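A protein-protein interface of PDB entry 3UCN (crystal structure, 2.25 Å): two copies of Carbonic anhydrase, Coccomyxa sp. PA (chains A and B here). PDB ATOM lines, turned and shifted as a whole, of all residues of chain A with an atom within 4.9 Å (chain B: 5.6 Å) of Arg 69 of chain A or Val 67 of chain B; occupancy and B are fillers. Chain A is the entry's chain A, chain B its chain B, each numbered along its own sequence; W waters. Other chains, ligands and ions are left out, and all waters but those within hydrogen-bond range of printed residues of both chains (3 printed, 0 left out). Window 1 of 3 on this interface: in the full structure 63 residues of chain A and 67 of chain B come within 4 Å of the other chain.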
ATOM      1  N   TYR A  44     -27.392 -15.650   0.520  1.00  0.00           N
ATOM      2  CA  TYR A  44     -26.769 -14.824   1.525  1.00  0.00           C
ATOM      3  C   TYR A  44     -25.660 -13.981   0.863  1.00  0.00           C
ATOM      4  O   TYR A  44     -24.832 -14.507   0.092  1.00  0.00           O
ATOM      5  CB  TYR A  44     -26.178 -15.707   2.554  1.00  0.00           C
ATOM      6  CG  TYR A  44     -25.192 -15.068   3.561  1.00  0.00           C
ATOM      7  CD1 TYR A  44     -25.607 -14.746   4.867  1.00  0.00           C
ATOM      8  CD2 TYR A  44     -23.862 -14.879   3.245  1.00  0.00           C
ATOM      9  CE1 TYR A  44     -24.706 -14.247   5.826  1.00  0.00           C
ATOM     10  CE2 TYR A  44     -22.951 -14.366   4.205  1.00  0.00           C
ATOM     11  CZ  TYR A  44     -23.390 -14.055   5.489  1.00  0.00           C
ATOM     12  OH  TYR A  44     -22.516 -13.564   6.395  1.00  0.00           O
ATOM     13  N   GLY A  46     -22.734 -11.541   2.227  1.00  0.00           N
ATOM     14  CA  GLY A  46     -22.041 -11.043   3.408  1.00  0.00           C
ATOM     15  C   GLY A  46     -20.588 -10.768   3.079  1.00  0.00           C
ATOM     16  O   GLY A  46     -20.184 -10.755   1.896  1.00  0.00           O
ATOM     17  N   CYS A  47     -19.768 -10.534   4.110  1.00  0.00           N
ATOM     18  CA  CYS A  47     -18.434 -10.015   3.888  1.00  0.00           C
ATOM     19  C   CYS A  47     -17.525 -11.197   3.767  1.00  0.00           C
ATOM     20  O   CYS A  47     -17.771 -12.247   4.388  1.00  0.00           O
ATOM     21  CB  CYS A  47     -18.036  -9.103   5.059  1.00  0.00           C
ATOM     22  SG  CYS A  47     -16.383  -8.267   4.764  1.00  0.00           S
ATOM     23  N   ALA A  48     -16.479 -11.023   2.974  1.00  0.00           N
ATOM     24  CA  ALA A  48     -15.360 -11.957   2.869  1.00  0.00           C
ATOM     25  C   ALA A  48     -14.590 -12.211   4.175  1.00  0.00           C
ATOM     26  O   ALA A  48     -13.855 -13.177   4.289  1.00  0.00           O
ATOM     27  CB  ALA A  48     -14.391 -11.469   1.853  1.00  0.00           C
ATOM     28  N   ASP A  49     -14.687 -11.295   5.117  1.00  0.00           N
ATOM     29  CA  ASP A  49     -14.064 -11.470   6.464  1.00  0.00           C
ATOM     30  C   ASP A  49     -14.043 -12.939   6.978  1.00  0.00           C
ATOM     31  O   ASP A  49     -15.084 -13.604   7.104  1.00  0.00           O
ATOM     32  CB  ASP A  49     -14.830 -10.607   7.471  1.00  0.00           C
ATOM     33  CG  ASP A  49     -14.106 -10.516   8.830  1.00  0.00           C
ATOM     34  OD1 ASP A  49     -14.262 -11.446   9.658  1.00  0.00           O
ATOM     35  OD2 ASP A  49     -13.370  -9.527   9.066  1.00  0.00           O
ATOM     36  N   SER A  50     -12.858 -13.423   7.320  1.00  0.00           N
ATOM     37  CA  SER A  50     -12.713 -14.831   7.836  1.00  0.00           C
ATOM     38  C   SER A  50     -13.521 -15.213   9.079  1.00  0.00           C
ATOM     39  O   SER A  50     -13.540 -16.383   9.442  1.00  0.00           O
ATOM     40  CB  SER A  50     -11.266 -15.122   8.163  1.00  0.00           C
ATOM     41  OG  SER A  50     -10.876 -14.305   9.258  1.00  0.00           O
ATOM     42  N   VAL A  52     -16.775 -14.879   9.465  1.00  0.00           N
ATOM     43  CA  VAL A  52     -18.204 -14.797   9.235  1.00  0.00           C
ATOM     44  C   VAL A  52     -18.602 -15.808   8.186  1.00  0.00           C
ATOM     45  O   VAL A  52     -18.641 -15.486   6.972  1.00  0.00           O
ATOM     46  CB  VAL A  52     -18.745 -13.368   8.797  1.00  0.00           C
ATOM     47  CG1 VAL A  52     -20.318 -13.265   9.052  1.00  0.00           C
ATOM     48  CG2 VAL A  52     -17.993 -12.228   9.472  1.00  0.00           C
ATOM     49  N   SER A  53     -18.934 -17.020   8.642  1.00  0.00           N
ATOM     50  CA  SER A  53     -19.284 -18.054   7.709  1.00  0.00           C
ATOM     51  C   SER A  53     -20.758 -18.416   7.784  1.00  0.00           C
ATOM     52  O   SER A  53     -21.195 -18.954   8.789  1.00  0.00           O
ATOM     53  CB  SER A  53     -18.398 -19.248   7.961  1.00  0.00           C
ATOM     54  OG  SER A  53     -19.003 -20.314   7.260  1.00  0.00           O
ATOM     55  N   PRO A  54     -21.559 -18.076   6.762  1.00  0.00           N
ATOM     56  CA  PRO A  54     -23.026 -18.208   6.959  1.00  0.00           C
ATOM     57  C   PRO A  54     -23.509 -19.617   7.343  1.00  0.00           C
ATOM     58  O   PRO A  54     -24.306 -19.758   8.285  1.00  0.00           O
ATOM     59  CB  PRO A  54     -23.621 -17.816   5.585  1.00  0.00           C
ATOM     60  CG  PRO A  54     -22.383 -17.782   4.619  1.00  0.00           C
ATOM     61  CD  PRO A  54     -21.222 -17.484   5.450  1.00  0.00           C
ATOM     62  N   VAL A  67     -24.310 -18.623  -1.622  1.00  0.00           N
ATOM     63  CA  VAL A  67     -23.471 -17.590  -0.948  1.00  0.00           C
ATOM     64  C   VAL A  67     -22.616 -16.659  -1.884  1.00  0.00           C
ATOM     65  O   VAL A  67     -21.776 -17.151  -2.662  1.00  0.00           O
ATOM     66  CB  VAL A  67     -22.561 -18.248   0.056  1.00  0.00           C
ATOM     67  CG1 VAL A  67     -21.561 -17.211   0.698  1.00  0.00           C
ATOM     68  CG2 VAL A  67     -23.385 -18.961   1.171  1.00  0.00           C
ATOM     69  N   GLN A  68     -22.817 -15.328  -1.792  1.00  0.00           N
ATOM     70  CA  GLN A  68     -21.867 -14.309  -2.344  1.00  0.00           C
ATOM     71  C   GLN A  68     -21.154 -13.746  -1.109  1.00  0.00           C
ATOM     72  O   GLN A  68     -21.810 -13.376  -0.165  1.00  0.00           O
ATOM     73  CB  GLN A  68     -22.642 -13.190  -3.082  1.00  0.00           C
ATOM     74  CG  GLN A  68     -21.984 -11.832  -3.166  1.00  0.00           C
ATOM     75  CD  GLN A  68     -20.788 -11.728  -4.208  1.00  0.00           C
ATOM     76  OE1 GLN A  68     -20.151 -10.711  -4.291  1.00  0.00           O
ATOM     77  NE2 GLN A  68     -20.528 -12.755  -4.963  1.00  0.00           N
ATOM     78  N   ARG A  69     -19.841 -13.715  -1.090  1.00  0.00           N
ATOM     79  CA  ARG A  69     -19.071 -13.061  -0.055  1.00  0.00           C
ATOM     80  C   ARG A  69     -18.020 -12.156  -0.740  1.00  0.00           C
ATOM     81  O   ARG A  69     -17.341 -12.611  -1.678  1.00  0.00           O
ATOM     82  CB  ARG A  69     -18.374 -14.071   0.864  1.00  0.00           C
ATOM     83  CG  ARG A  69     -19.359 -14.605   1.896  1.00  0.00           C
ATOM     84  CD  ARG A  69     -18.774 -15.717   2.780  1.00  0.00           C
ATOM     85  NE  ARG A  69     -17.804 -15.168   3.727  1.00  0.00           N
ATOM     86  CZ  ARG A  69     -17.051 -15.917   4.546  1.00  0.00           C
ATOM     87  NH1 ARG A  69     -17.205 -17.268   4.607  1.00  0.00           N
ATOM     88  NH2 ARG A  69     -16.193 -15.302   5.367  1.00  0.00           N
ATOM     89  N   ASN A  70     -17.988 -10.861  -0.358  1.00  0.00           N
ATOM     90  CA  ASN A  70     -17.079  -9.895  -0.991  1.00  0.00           C
ATOM     91  C   ASN A  70     -16.614  -8.901   0.074  1.00  0.00           C
ATOM     92  O   ASN A  70     -17.161  -8.908   1.185  1.00  0.00           O
ATOM     93  CB  ASN A  70     -17.716  -9.214  -2.222  1.00  0.00           C
ATOM     94  CG  ASN A  70     -18.875  -8.282  -1.870  1.00  0.00           C
ATOM     95  OD1 ASN A  70     -18.731  -7.453  -1.017  1.00  0.00           O
ATOM     96  ND2 ASN A  70     -20.055  -8.410  -2.580  1.00  0.00           N
ATOM     97  N   VAL A  71     -15.601  -8.089  -0.238  1.00  0.00           N
ATOM     98  CA  VAL A  71     -15.052  -7.179   0.750  1.00  0.00           C
ATOM     99  C   VAL A  71     -16.096  -6.067   1.077  1.00  0.00           C
ATOM    100  O   VAL A  71     -16.368  -5.197   0.280  1.00  0.00           O
ATOM    101  CB  VAL A  71     -13.732  -6.609   0.251  1.00  0.00           C
ATOM    102  CG1 VAL A  71     -13.258  -5.515   1.144  1.00  0.00           C
ATOM    103  CG2 VAL A  71     -12.701  -7.723   0.179  1.00  0.00           C
ATOM    104  N   LEU B  43      -6.758 -17.817   1.986  1.00  0.00           N
ATOM    105  CA  LEU B  43      -7.828 -17.237   1.153  1.00  0.00           C
ATOM    106  C   LEU B  43      -8.357 -18.399   0.363  1.00  0.00           C
ATOM    107  O   LEU B  43      -7.583 -19.172  -0.184  1.00  0.00           O
ATOM    108  CB  LEU B  43      -7.321 -16.131   0.195  1.00  0.00           C
ATOM    109  CG  LEU B  43      -8.245 -15.691  -0.985  1.00  0.00           C
ATOM    110  CD1 LEU B  43      -9.384 -14.859  -0.495  1.00  0.00           C
ATOM    111  CD2 LEU B  43      -7.419 -14.923  -2.040  1.00  0.00           C
ATOM    112  N   TYR B  44      -9.674 -18.484   0.310  1.00  0.00           N
ATOM    113  CA  TYR B  44     -10.381 -19.469  -0.454  1.00  0.00           C
ATOM    114  C   TYR B  44     -11.199 -18.762  -1.531  1.00  0.00           C
ATOM    115  O   TYR B  44     -11.959 -17.819  -1.257  1.00  0.00           O
ATOM    116  CB  TYR B  44     -11.379 -20.129   0.483  1.00  0.00           C
ATOM    117  CG  TYR B  44     -12.270 -21.139  -0.165  1.00  0.00           C
ATOM    118  CD1 TYR B  44     -11.910 -22.477  -0.241  1.00  0.00           C
ATOM    119  CD2 TYR B  44     -13.493 -20.762  -0.650  1.00  0.00           C
ATOM    120  CE1 TYR B  44     -12.754 -23.414  -0.840  1.00  0.00           C
ATOM    121  CE2 TYR B  44     -14.361 -21.664  -1.229  1.00  0.00           C
ATOM    122  CZ  TYR B  44     -13.991 -22.995  -1.321  1.00  0.00           C
ATOM    123  OH  TYR B  44     -14.881 -23.844  -1.902  1.00  0.00           O
ATOM    124  N   PRO B  54     -16.655 -23.567   2.604  1.00  0.00           N
ATOM    125  CA  PRO B  54     -15.287 -23.938   3.018  1.00  0.00           C
ATOM    126  C   PRO B  54     -15.052 -24.133   4.512  1.00  0.00           C
ATOM    127  O   PRO B  54     -14.385 -25.103   4.888  1.00  0.00           O
ATOM    128  CB  PRO B  54     -14.423 -22.793   2.509  1.00  0.00           C
ATOM    129  CG  PRO B  54     -15.412 -21.610   2.259  1.00  0.00           C
ATOM    130  CD  PRO B  54     -16.668 -22.334   1.792  1.00  0.00           C
ATOM    131  N   VAL B  65     -10.206 -18.796   7.442  1.00  0.00           N
ATOM    132  CA  VAL B  65     -10.199 -18.724   5.988  1.00  0.00           C
ATOM    133  C   VAL B  65     -11.006 -17.494   5.547  1.00  0.00           C
ATOM    134  O   VAL B  65     -12.224 -17.371   5.823  1.00  0.00           O
ATOM    135  CB  VAL B  65     -10.683 -20.081   5.309  1.00  0.00           C
ATOM    136  CG1 VAL B  65     -12.059 -20.400   5.744  1.00  0.00           C
ATOM    137  CG2 VAL B  65     -10.612 -20.025   3.735  1.00  0.00           C
ATOM    138  N   PHE B  66     -10.329 -16.579   4.850  1.00  0.00           N
ATOM    139  CA  PHE B  66     -11.037 -15.420   4.254  1.00  0.00           C
ATOM    140  C   PHE B  66     -11.681 -15.909   2.909  1.00  0.00           C
ATOM    141  O   PHE B  66     -11.014 -16.608   2.101  1.00  0.00           O
ATOM    142  CB  PHE B  66      -9.972 -14.353   4.034  1.00  0.00           C
ATOM    143  CG  PHE B  66     -10.491 -12.976   3.665  1.00  0.00           C
ATOM    144  CD1 PHE B  66     -10.511 -11.974   4.605  1.00  0.00           C
ATOM    145  CD2 PHE B  66     -10.785 -12.645   2.317  1.00  0.00           C
ATOM    146  CE1 PHE B  66     -10.853 -10.664   4.271  1.00  0.00           C
ATOM    147  CE2 PHE B  66     -11.153 -11.320   1.961  1.00  0.00           C
ATOM    148  CZ  PHE B  66     -11.187 -10.335   2.928  1.00  0.00           C
ATOM    149  N   VAL B  67     -12.923 -15.536   2.629  1.00  0.00           N
ATOM    150  CA  VAL B  67     -13.615 -16.191   1.514  1.00  0.00           C
ATOM    151  C   VAL B  67     -14.122 -15.301   0.369  1.00  0.00           C
ATOM    152  O   VAL B  67     -14.879 -14.330   0.609  1.00  0.00           O
ATOM    153  CB  VAL B  67     -14.791 -17.051   2.084  1.00  0.00           C
ATOM    154  CG1 VAL B  67     -15.642 -17.606   0.959  1.00  0.00           C
ATOM    155  CG2 VAL B  67     -14.252 -18.179   2.983  1.00  0.00           C
ATOM    156  N   GLN B  68     -13.768 -15.654  -0.867  1.00  0.00           N
ATOM    157  CA  GLN B  68     -14.504 -15.175  -2.049  1.00  0.00           C
ATOM    158  C   GLN B  68     -15.359 -16.330  -2.633  1.00  0.00           C
ATOM    159  O   GLN B  68     -14.848 -17.417  -2.895  1.00  0.00           O
ATOM    160  CB  GLN B  68     -13.490 -14.721  -3.098  1.00  0.00           C
ATOM    161  CG  GLN B  68     -13.939 -14.576  -4.546  1.00  0.00           C
ATOM    162  CD  GLN B  68     -14.926 -13.462  -4.982  1.00  0.00           C
ATOM    163  OE1 GLN B  68     -15.381 -13.509  -6.125  1.00  0.00           O
ATOM    164  NE2 GLN B  68     -15.240 -12.487  -4.131  1.00  0.00           N
ATOM    165  N   ARG B  69     -16.645 -16.114  -2.884  1.00  0.00           N
ATOM    166  CA  ARG B  69     -17.459 -17.110  -3.610  1.00  0.00           C
ATOM    167  C   ARG B  69     -18.254 -16.412  -4.696  1.00  0.00           C
ATOM    168  O   ARG B  69     -18.870 -15.382  -4.465  1.00  0.00           O
ATOM    169  CB  ARG B  69     -18.360 -17.922  -2.661  1.00  0.00           C
ATOM    170  CG  ARG B  69     -17.558 -18.899  -1.811  1.00  0.00           C
ATOM    171  CD  ARG B  69     -18.416 -19.511  -0.633  1.00  0.00           C
ATOM    172  NE  ARG B  69     -19.491 -20.342  -1.184  1.00  0.00           N
ATOM    173  CZ  ARG B  69     -20.419 -20.996  -0.458  1.00  0.00           C
ATOM    174  NH1 ARG B  69     -20.441 -20.950   0.873  1.00  0.00           N
ATOM    175  NH2 ARG B  69     -21.320 -21.714  -1.097  1.00  0.00           N
ATOM    176  N   ASN B  81     -14.190  -7.256  -7.703  1.00  0.00           N
ATOM    177  CA  ASN B  81     -14.806  -7.959  -6.546  1.00  0.00           C
ATOM    178  C   ASN B  81     -13.842  -9.065  -6.092  1.00  0.00           C
ATOM    179  O   ASN B  81     -13.297  -9.027  -4.963  1.00  0.00           O
ATOM    180  CB  ASN B  81     -16.187  -8.557  -6.971  1.00  0.00           C
ATOM    181  CG  ASN B  81     -16.886  -9.341  -5.855  1.00  0.00           C
ATOM    182  OD1 ASN B  81     -16.249 -10.021  -5.059  1.00  0.00           O
ATOM    183  ND2 ASN B  81     -18.212  -9.294  -5.846  1.00  0.00           N
ATOM    184  N   CYS B  85     -10.581  -9.038  -2.996  1.00  0.00           N
ATOM    185  CA  CYS B  85     -10.387 -10.125  -2.035  1.00  0.00           C
ATOM    186  C   CYS B  85      -8.921 -10.565  -2.080  1.00  0.00           C
ATOM    187  O   CYS B  85      -8.273 -10.702  -1.043  1.00  0.00           O
ATOM    188  CB  CYS B  85     -11.292 -11.297  -2.368  1.00  0.00           C
ATOM    189  SG  CYS B  85     -12.968 -11.049  -1.813  1.00  0.00           S
HETATM  190  O   HOH W   1     -12.700 -19.336   9.027  1.00  0.00           O
HETATM  191  O   HOH W   2     -15.046 -17.815   6.563  1.00  0.00           O
HETATM  192  O   HOH W   3     -14.664  -7.945  -2.845  1.00  0.00           O
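The side-chain amide nitrogen of Gln 68 of chain A sits at hydrogen-bond distance from the backbone carbonyl oxygen of Arg 69 of chain B.
The side-chain amide oxygen (OE1) of Gln 68 of chain A sits at hydrogen-bond distance from the side-chain amide nitrogen (ND2) of Asn 81 of chain B (2.9 Å).
The backbone carbonyl oxygen (O) of Ala 48 of chain A is in hydrogen-bond range of the backbone NH (N) of Val 67 of chain B, 3.0 Å away.
The backbone carbonyl oxygen (O) of Arg 69 of chain A lies within hydrogen-bond range of the side-chain amide nitrogen (NE2) of Gln 68 of chain B, 3.2 Å away.
Val 67 of chain A touches Arg 69 of chain B, and with the chains exchanged Arg 69 of chain A touches Val 67 of chain B.
Gln 68 of chain A touches Arg 69 of chain B, and with the chains exchanged Arg 69 of chain A touches Gln 68 of chain B.
Arg 69 of chain A touches its own counterpart, Arg 69 of chain B.
Positions printed for both chains: 44, 54, 67, 68 and 69.
Of the 14 pairs that touch across the chains among the printed residues, 5 have their exchanged pair printed and touching as well.
Water W3 lies within hydrogen-bond range of O of Asn 81 of chain B (2.7 Å), N of Val 71 of chain A (2.8 Å) and SG of Cys 85 of chain B (3.7 Å).
Water W2 bridges the backbone carbonyl oxygen of Val 65 of chain B (3.0 Å) and the guanidinium group of Arg 69 of chain A (3.0 Å).
Water W1 bridges the backbone NH of Val 65 of chain B (3.0 Å) and the backbone carbonyl oxygen of Ser 50 of chain A (3.1 Å).
Among the printed residues, pairs that only touch across the chains: Ala 48 of chain A with Phe 66 of chain B (3.2 Å), Ala 48 of chain A with Cys 85 of chain B (3.95 Å), Asp 49 of chain A with Phe 66 of chain B (3.97 Å), Ser 50 of chain A with Val 65 of chain B (3.3 Å), Ser 50 of chain A with Phe 66 of chain B (3.7 Å), Val 67 of chain A with Arg 69 of chain B (3.5 Å), Arg 69 of chain A with Val 67 of chain B (3.5 Å), Arg 69 of chain A with Arg 69 of chain B (3.8 Å), Asn 70 of chain A with Asn 81 of chain B (3.3 Å) and Val 71 of chain A with Cys 85 of chain B (3.9 Å).
Of the 10 printed residues of chain B, 7 touch a printed residue of chain A.
Printed residues of chain A that touch a printed residue of chain B: Ala 48, Asp 49, Ser 50, Val 67, Gln 68, Arg 69, Asn 70 and Val 71.
Arg 69 of chain A touches just these residues of chain B: Val 67, Gln 68 and Arg 69.
Of chain A, only Ala 48 and Arg 69 come within 4 Å of Val 67 of chain B.
Of the printed residues of chain A, Arg 69 of chain B touches Val 67 (3.5 Å), Gln 68 (3.1 Å) and Arg 69 (3.8 Å).
Of the printed residues of chain A, Cys 85 of chain B touches Ala 48 and Val 71.
Of the printed residues of chain B, Ser 50 of chain A touches Val 65 (3.3 Å) and Phe 66 (3.7 Å).
Printed residues of chain A within 4 Å of Asn 81 of chain B: Gln 68 (2.9 Å) and Asn 70 (3.3 Å).
Printed residues of chain B within 4 Å of Asp 49 of chain A: Phe 66 (3.97 Å).
NH2 of Arg 69 of chain A lies within hydrogen-bond range of O of Asp 49 of chain A.
The guanidinium group (NE) of Arg 69 of chain A lies within hydrogen-bond range of the backbone carbonyl oxygen (O) of Cys 47 of chain A, 3.0 Å away.
O of Asn 81 of chain B lies within hydrogen-bond range of SG of Cys 85 of chain B (3.8 Å).
NE2 of Gln 68 of chain B is in hydrogen-bond range of OD1 of Asn 81 of chain B (2.8 Å).
N of Ala 48 of chain A sits at hydrogen-bond distance from O of Asn 70 of chain A, 2.9 Å away.
O of Tyr 44 of chain A is in hydrogen-bond range of N of Gln 68 of chain A (2.9 Å).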
